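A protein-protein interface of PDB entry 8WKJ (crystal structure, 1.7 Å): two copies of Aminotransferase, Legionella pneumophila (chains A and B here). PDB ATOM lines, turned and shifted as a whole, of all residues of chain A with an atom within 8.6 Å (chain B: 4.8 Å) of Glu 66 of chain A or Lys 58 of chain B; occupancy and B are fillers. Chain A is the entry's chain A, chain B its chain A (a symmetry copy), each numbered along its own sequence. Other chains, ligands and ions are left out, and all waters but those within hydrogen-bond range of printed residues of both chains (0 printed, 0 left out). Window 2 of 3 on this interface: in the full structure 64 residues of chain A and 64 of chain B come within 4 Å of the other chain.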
ATOM      1  N   LEU A  59     -25.667   4.915  19.018  1.00  0.00           N
ATOM      2  CA  LEU A  59     -26.966   5.383  19.490  1.00  0.00           C
ATOM      3  C   LEU A  59     -27.921   4.220  19.713  1.00  0.00           C
ATOM      4  O   LEU A  59     -28.733   4.245  20.647  1.00  0.00           O
ATOM      5  CB  LEU A  59     -27.562   6.376  18.495  1.00  0.00           C
ATOM      6  CG  LEU A  59     -26.864   7.733  18.438  1.00  0.00           C
ATOM      7  CD1 LEU A  59     -27.538   8.618  17.388  1.00  0.00           C
ATOM      8  CD2 LEU A  59     -26.870   8.404  19.811  1.00  0.00           C
ATOM      9  N   ALA A  60     -27.846   3.197  18.856  1.00  0.00           N
ATOM     10  CA  ALA A  60     -28.684   2.017  19.034  1.00  0.00           C
ATOM     11  C   ALA A  60     -28.298   1.258  20.292  1.00  0.00           C
ATOM     12  O   ALA A  60     -29.167   0.703  20.979  1.00  0.00           O
ATOM     13  CB  ALA A  60     -28.586   1.101  17.816  1.00  0.00           C
ATOM     14  N   ALA A  61     -27.000   1.208  20.602  1.00  0.00           N
ATOM     15  CA  ALA A  61     -26.577   0.554  21.835  1.00  0.00           C
ATOM     16  C   ALA A  61     -27.068   1.329  23.049  1.00  0.00           C
ATOM     17  O   ALA A  61     -27.590   0.738  24.002  1.00  0.00           O
ATOM     18  CB  ALA A  61     -25.057   0.402  21.861  1.00  0.00           C
ATOM     19  N   ILE A  62     -26.945   2.654  23.016  1.00  0.00           N
ATOM     20  CA  ILE A  62     -27.409   3.456  24.139  1.00  0.00           C
ATOM     21  C   ILE A  62     -28.918   3.305  24.312  1.00  0.00           C
ATOM     22  O   ILE A  62     -29.415   3.179  25.439  1.00  0.00           O
ATOM     23  CB  ILE A  62     -26.982   4.920  23.950  1.00  0.00           C
ATOM     24  CG1 ILE A  62     -25.459   5.026  24.074  1.00  0.00           C
ATOM     25  CG2 ILE A  62     -27.673   5.819  24.977  1.00  0.00           C
ATOM     26  CD1 ILE A  62     -24.868   6.366  23.602  1.00  0.00           C
ATOM     27  N   SER A  63     -29.669   3.279  23.204  1.00  0.00           N
ATOM     28  CA  SER A  63     -31.117   3.094  23.299  1.00  0.00           C
ATOM     29  C   SER A  63     -31.463   1.752  23.928  1.00  0.00           C
ATOM     30  O   SER A  63     -32.438   1.646  24.686  1.00  0.00           O
ATOM     31  CB  SER A  63     -31.767   3.199  21.916  1.00  0.00           C
ATOM     32  OG  SER A  63     -31.720   4.528  21.431  1.00  0.00           O
ATOM     33  N   ALA A  64     -30.687   0.708  23.605  1.00  0.00           N
ATOM     34  CA  ALA A  64     -30.912  -0.608  24.203  1.00  0.00           C
ATOM     35  C   ALA A  64     -30.633  -0.593  25.701  1.00  0.00           C
ATOM     36  O   ALA A  64     -31.350  -1.231  26.480  1.00  0.00           O
ATOM     37  CB  ALA A  64     -30.038  -1.656  23.506  1.00  0.00           C
ATOM     38  N   ILE A  65     -29.580   0.111  26.121  1.00  0.00           N
ATOM     39  CA  ILE A  65     -29.277   0.216  27.547  1.00  0.00           C
ATOM     40  C   ILE A  65     -30.423   0.908  28.266  1.00  0.00           C
ATOM     41  O   ILE A  65     -30.908   0.445  29.305  1.00  0.00           O
ATOM     42  CB  ILE A  65     -27.954   0.976  27.752  1.00  0.00           C
ATOM     43  CG1 ILE A  65     -26.776   0.162  27.209  1.00  0.00           C
ATOM     44  CG2 ILE A  65     -27.743   1.320  29.220  1.00  0.00           C
ATOM     45  CD1 ILE A  65     -25.467   0.953  27.227  1.00  0.00           C
ATOM     46  N   GLU A  66     -30.886   2.023  27.704  1.00  0.00           N
ATOM     47  CA  GLU A  66     -31.965   2.774  28.332  1.00  0.00           C
ATOM     48  C   GLU A  66     -33.254   1.965  28.364  1.00  0.00           C
ATOM     49  O   GLU A  66     -34.048   2.098  29.302  1.00  0.00           O
ATOM     50  CB  GLU A  66     -32.155   4.105  27.595  1.00  0.00           C
ATOM     51  CG  GLU A  66     -30.965   5.035  27.774  1.00  0.00           C
ATOM     52  CD  GLU A  66     -31.042   6.293  26.928  1.00  0.00           C
ATOM     53  OE1 GLU A  66     -31.848   6.336  25.975  1.00  0.00           O
ATOM     54  OE2 GLU A  66     -30.287   7.245  27.225  1.00  0.00           O
ATOM     55  N   ALA A  67     -33.469   1.102  27.373  1.00  0.00           N
ATOM     56  CA  ALA A  67     -34.686   0.296  27.347  1.00  0.00           C
ATOM     57  C   ALA A  67     -34.626  -0.920  28.266  1.00  0.00           C
ATOM     58  O   ALA A  67     -35.632  -1.625  28.394  1.00  0.00           O
ATOM     59  CB  ALA A  67     -34.985  -0.163  25.917  1.00  0.00           C
ATOM     60  N   GLY A  68     -33.487  -1.190  28.900  1.00  0.00           N
ATOM     61  CA  GLY A  68     -33.384  -2.344  29.776  1.00  0.00           C
ATOM     62  C   GLY A  68     -33.126  -3.658  29.073  1.00  0.00           C
ATOM     63  O   GLY A  68     -33.514  -4.719  29.583  1.00  0.00           O
ATOM     64  N   ASP A  69     -32.462  -3.620  27.918  1.00  0.00           N
ATOM     65  CA  ASP A  69     -32.109  -4.819  27.159  1.00  0.00           C
ATOM     66  C   ASP A  69     -30.848  -5.458  27.746  1.00  0.00           C
ATOM     67  O   ASP A  69     -29.821  -5.618  27.084  1.00  0.00           O
ATOM     68  CB  ASP A  69     -31.911  -4.469  25.692  1.00  0.00           C
ATOM     69  CG  ASP A  69     -32.337  -5.578  24.774  1.00  0.00           C
ATOM     70  OD1 ASP A  69     -32.356  -6.745  25.226  1.00  0.00           O
ATOM     71  OD2 ASP A  69     -32.641  -5.295  23.598  1.00  0.00           O
ATOM     72  N   THR A  70     -30.964  -5.840  29.019  1.00  0.00           N
ATOM     73  CA  THR A  70     -29.830  -6.241  29.842  1.00  0.00           C
ATOM     74  C   THR A  70     -29.937  -7.685  30.320  1.00  0.00           C
ATOM     75  O   THR A  70     -29.294  -8.051  31.316  1.00  0.00           O
ATOM     76  CB  THR A  70     -29.729  -5.310  31.044  1.00  0.00           C
ATOM     77  OG1 THR A  70     -30.967  -5.364  31.769  1.00  0.00           O
ATOM     78  CG2 THR A  70     -29.472  -3.871  30.593  1.00  0.00           C
ATOM     79  N   ILE A 282     -26.455  -5.901  24.726  1.00  0.00           N
ATOM     80  CA  ILE A 282     -26.329  -4.552  24.177  1.00  0.00           C
ATOM     81  C   ILE A 282     -25.576  -4.596  22.857  1.00  0.00           C
ATOM     82  O   ILE A 282     -25.948  -3.929  21.883  1.00  0.00           O
ATOM     83  CB  ILE A 282     -25.620  -3.643  25.197  1.00  0.00           C
ATOM     84  CG1 ILE A 282     -26.426  -3.571  26.504  1.00  0.00           C
ATOM     85  CG2 ILE A 282     -25.347  -2.277  24.591  1.00  0.00           C
ATOM     86  CD1 ILE A 282     -27.882  -3.139  26.320  1.00  0.00           C
ATOM     87  N   ASP B  52     -33.909  -4.406  36.458  1.00  0.00           N
ATOM     88  CA  ASP B  52     -32.972  -3.934  35.439  1.00  0.00           C
ATOM     89  C   ASP B  52     -31.603  -3.660  36.068  1.00  0.00           C
ATOM     90  O   ASP B  52     -31.450  -3.570  37.292  1.00  0.00           O
ATOM     91  CB  ASP B  52     -33.514  -2.656  34.784  1.00  0.00           C
ATOM     92  CG  ASP B  52     -32.931  -2.377  33.394  1.00  0.00           C
ATOM     93  OD1 ASP B  52     -32.010  -3.079  32.922  1.00  0.00           O
ATOM     94  OD2 ASP B  52     -33.438  -1.427  32.761  1.00  0.00           O
ATOM     95  N   THR B  53     -30.597  -3.534  35.212  1.00  0.00           N
ATOM     96  CA  THR B  53     -29.285  -3.104  35.667  1.00  0.00           C
ATOM     97  C   THR B  53     -29.406  -1.756  36.376  1.00  0.00           C
ATOM     98  O   THR B  53     -30.069  -0.848  35.854  1.00  0.00           O
ATOM     99  CB  THR B  53     -28.337  -2.991  34.470  1.00  0.00           C
ATOM    100  OG1 THR B  53     -28.200  -4.282  33.861  1.00  0.00           O
ATOM    101  CG2 THR B  53     -26.974  -2.480  34.915  1.00  0.00           C
ATOM    102  N   PRO B  54     -28.794  -1.585  37.551  1.00  0.00           N
ATOM    103  CA  PRO B  54     -28.863  -0.297  38.257  1.00  0.00           C
ATOM    104  C   PRO B  54     -28.413   0.880  37.392  1.00  0.00           C
ATOM    105  O   PRO B  54     -27.526   0.760  36.538  1.00  0.00           O
ATOM    106  CB  PRO B  54     -27.928  -0.507  39.456  1.00  0.00           C
ATOM    107  CG  PRO B  54     -28.027  -1.999  39.738  1.00  0.00           C
ATOM    108  CD  PRO B  54     -28.124  -2.626  38.348  1.00  0.00           C
ATOM    109  N   GLN B  55     -29.042   2.039  37.632  1.00  0.00           N
ATOM    110  CA  GLN B  55     -28.844   3.199  36.762  1.00  0.00           C
ATOM    111  C   GLN B  55     -27.388   3.665  36.734  1.00  0.00           C
ATOM    112  O   GLN B  55     -26.886   4.078  35.680  1.00  0.00           O
ATOM    113  CB  GLN B  55     -29.767   4.343  37.205  1.00  0.00           C
ATOM    114  CG  GLN B  55     -29.616   5.635  36.400  1.00  0.00           C
ATOM    115  CD  GLN B  55     -30.038   5.501  34.944  1.00  0.00           C
ATOM    116  OE1 GLN B  55     -30.578   4.473  34.527  1.00  0.00           O
ATOM    117  NE2 GLN B  55     -29.807   6.555  34.168  1.00  0.00           N
ATOM    118  N   HIS B  56     -26.687   3.627  37.873  1.00  0.00           N
ATOM    119  CA  HIS B  56     -25.310   4.123  37.849  1.00  0.00           C
ATOM    120  C   HIS B  56     -24.414   3.240  36.991  1.00  0.00           C
ATOM    121  O   HIS B  56     -23.452   3.731  36.388  1.00  0.00           O
ATOM    122  CB  HIS B  56     -24.739   4.246  39.264  1.00  0.00           C
ATOM    123  CG  HIS B  56     -24.544   2.939  39.969  1.00  0.00           C
ATOM    124  ND1 HIS B  56     -25.595   2.153  40.391  1.00  0.00           N
ATOM    125  CD2 HIS B  56     -23.414   2.294  40.352  1.00  0.00           C
ATOM    126  CE1 HIS B  56     -25.124   1.078  40.998  1.00  0.00           C
ATOM    127  NE2 HIS B  56     -23.804   1.140  40.988  1.00  0.00           N
ATOM    128  N   ILE B  57     -24.718   1.945  36.917  1.00  0.00           N
ATOM    129  CA  ILE B  57     -23.967   1.064  36.026  1.00  0.00           C
ATOM    130  C   ILE B  57     -24.307   1.359  34.568  1.00  0.00           C
ATOM    131  O   ILE B  57     -23.417   1.436  33.711  1.00  0.00           O
ATOM    132  CB  ILE B  57     -24.232  -0.407  36.394  1.00  0.00           C
ATOM    133  CG1 ILE B  57     -23.698  -0.682  37.805  1.00  0.00           C
ATOM    134  CG2 ILE B  57     -23.578  -1.337  35.356  1.00  0.00           C
ATOM    135  CD1 ILE B  57     -24.317  -1.894  38.485  1.00  0.00           C
ATOM    136  N   LYS B  58     -25.597   1.528  34.260  1.00  0.00           N
ATOM    137  CA  LYS B  58     -25.992   1.920  32.911  1.00  0.00           C
ATOM    138  C   LYS B  58     -25.286   3.197  32.479  1.00  0.00           C
ATOM    139  O   LYS B  58     -24.795   3.293  31.349  1.00  0.00           O
ATOM    140  CB  LYS B  58     -27.505   2.125  32.844  1.00  0.00           C
ATOM    141  CG  LYS B  58     -28.335   0.860  32.846  1.00  0.00           C
ATOM    142  CD  LYS B  58     -29.807   1.275  32.690  1.00  0.00           C
ATOM    143  CE  LYS B  58     -30.720   0.094  32.514  1.00  0.00           C
ATOM    144  NZ  LYS B  58     -32.027   0.569  31.948  1.00  0.00           N
ATOM    145  N   LEU B  59     -25.229   4.193  33.369  1.00  0.00           N
ATOM    146  CA  LEU B  59     -24.621   5.468  33.005  1.00  0.00           C
ATOM    147  C   LEU B  59     -23.140   5.304  32.699  1.00  0.00           C
ATOM    148  O   LEU B  59     -22.605   5.977  31.809  1.00  0.00           O
ATOM    149  CB  LEU B  59     -24.822   6.486  34.126  1.00  0.00           C
ATOM    150  CG  LEU B  59     -26.256   6.984  34.299  1.00  0.00           C
ATOM    151  CD1 LEU B  59     -26.323   7.970  35.466  1.00  0.00           C
ATOM    152  CD2 LEU B  59     -26.768   7.620  33.008  1.00  0.00           C
ATOM    153  N   ALA B  60     -22.460   4.421  33.438  1.00  0.00           N
ATOM    154  CA  ALA B  60     -21.050   4.160  33.169  1.00  0.00           C
ATOM    155  C   ALA B  60     -20.867   3.483  31.822  1.00  0.00           C
ATOM    156  O   ALA B  60     -19.884   3.750  31.117  1.00  0.00           O
ATOM    157  CB  ALA B  60     -20.445   3.300  34.276  1.00  0.00           C
ATOM    158  N   ALA B  61     -21.793   2.594  31.453  1.00  0.00           N
ATOM    159  CA  ALA B  61     -21.708   1.965  30.140  1.00  0.00           C
ATOM    160  C   ALA B  61     -21.930   2.991  29.038  1.00  0.00           C
ATOM    161  O   ALA B  61     -21.187   3.023  28.051  1.00  0.00           O
ATOM    162  CB  ALA B  61     -22.714   0.820  30.033  1.00  0.00           C
ATOM    163  N   ILE B  62     -22.924   3.861  29.209  1.00  0.00           N
ATOM    164  CA  ILE B  62     -23.180   4.878  28.199  1.00  0.00           C
ATOM    165  C   ILE B  62     -21.984   5.818  28.075  1.00  0.00           C
ATOM    166  O   ILE B  62     -21.583   6.188  26.964  1.00  0.00           O
ATOM    167  CB  ILE B  62     -24.484   5.625  28.526  1.00  0.00           C
ATOM    168  CG1 ILE B  62     -25.672   4.674  28.350  1.00  0.00           C
ATOM    169  CG2 ILE B  62     -24.637   6.857  27.632  1.00  0.00           C
ATOM    170  CD1 ILE B  62     -26.998   5.189  28.938  1.00  0.00           C
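The side-chain hydroxyl of Thr 70 of chain A lies within hydrogen-bond range of the backbone carbonyl oxygen of Gly 68 of chain A (3.4 Å).
The side-chain carboxylate (OD2) of Asp 52 of chain B lies within salt-bridge range of the side-chain amino group (NZ) of Lys 58 of chain B (2.6 Å).
Among the printed residues, merely in contact across the chains: Gly 68 of chain A with Asp 52 of chain B (3.1 Å), Thr 70 of chain A with Thr 53 of chain B (3.4 Å), Glu 66 of chain A with Lys 58 of chain B (3.7 Å), Gly 68 of chain A with Lys 58 of chain B (3.8 Å), Ile 65 of chain A with Ile 62 of chain B (3.9 Å) and Ile 65 of chain A with Ala 61 of chain B (3.9 Å).
The backbone carbonyl oxygen (O) of Ile 65 of chain A is in hydrogen-bond range of the side-chain amino group (NZ) of Lys 58 of chain B, at 2.9 Å.
The side-chain hydroxyl (OG1) of Thr 70 of chain A sits at hydrogen-bond distance from the side-chain carboxylate (OD1) of Asp 52 of chain B (2.8 Å).
Positions printed for both chains: 59, 60, 61 and 62.
Of the 8 pairs that touch across the chains among the printed residues, none has its exchanged pair printed and touching as well.
Printed residues of chain B within 4 Å of Ile 65 of chain A: Lys 58 (2.9 Å), Ala 61 (3.9 Å) and Ile 62 (3.9 Å).
Glu 66 of chain A touches just one residue of chain B: Lys 58.
Of the printed residues of chain B, Gly 68 of chain A touches Asp 52 (3.1 Å) and Lys 58 (3.8 Å).
Of the printed residues of chain A, Thr 53 of chain B touches Thr 70.
Lys 58 of chain B touches just these residues of chain A: Ile 65, Glu 66 and Gly 68.
The nearest residue of chain B that does not touch Glu 66 of chain A is Ile 62 of chain B (4.1 Å).
Hydrophobic or aromatic side chains of chain B within 4 Å of the printed part of chain A: Ala 61 and Ile 62.
Of the 13 printed residues of chain A, 4 touch a printed residue of chain B.
Hydrophobic or aromatic side chains of chain A that line the printed part of chain B: Ile 65.
Among the printed residues, 8 pairs touch across the chains.
Among the printed residues, no Asp or Glu carboxylate lies within 4 Å of a Lys or Arg side-chain nitrogen of the other chain.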
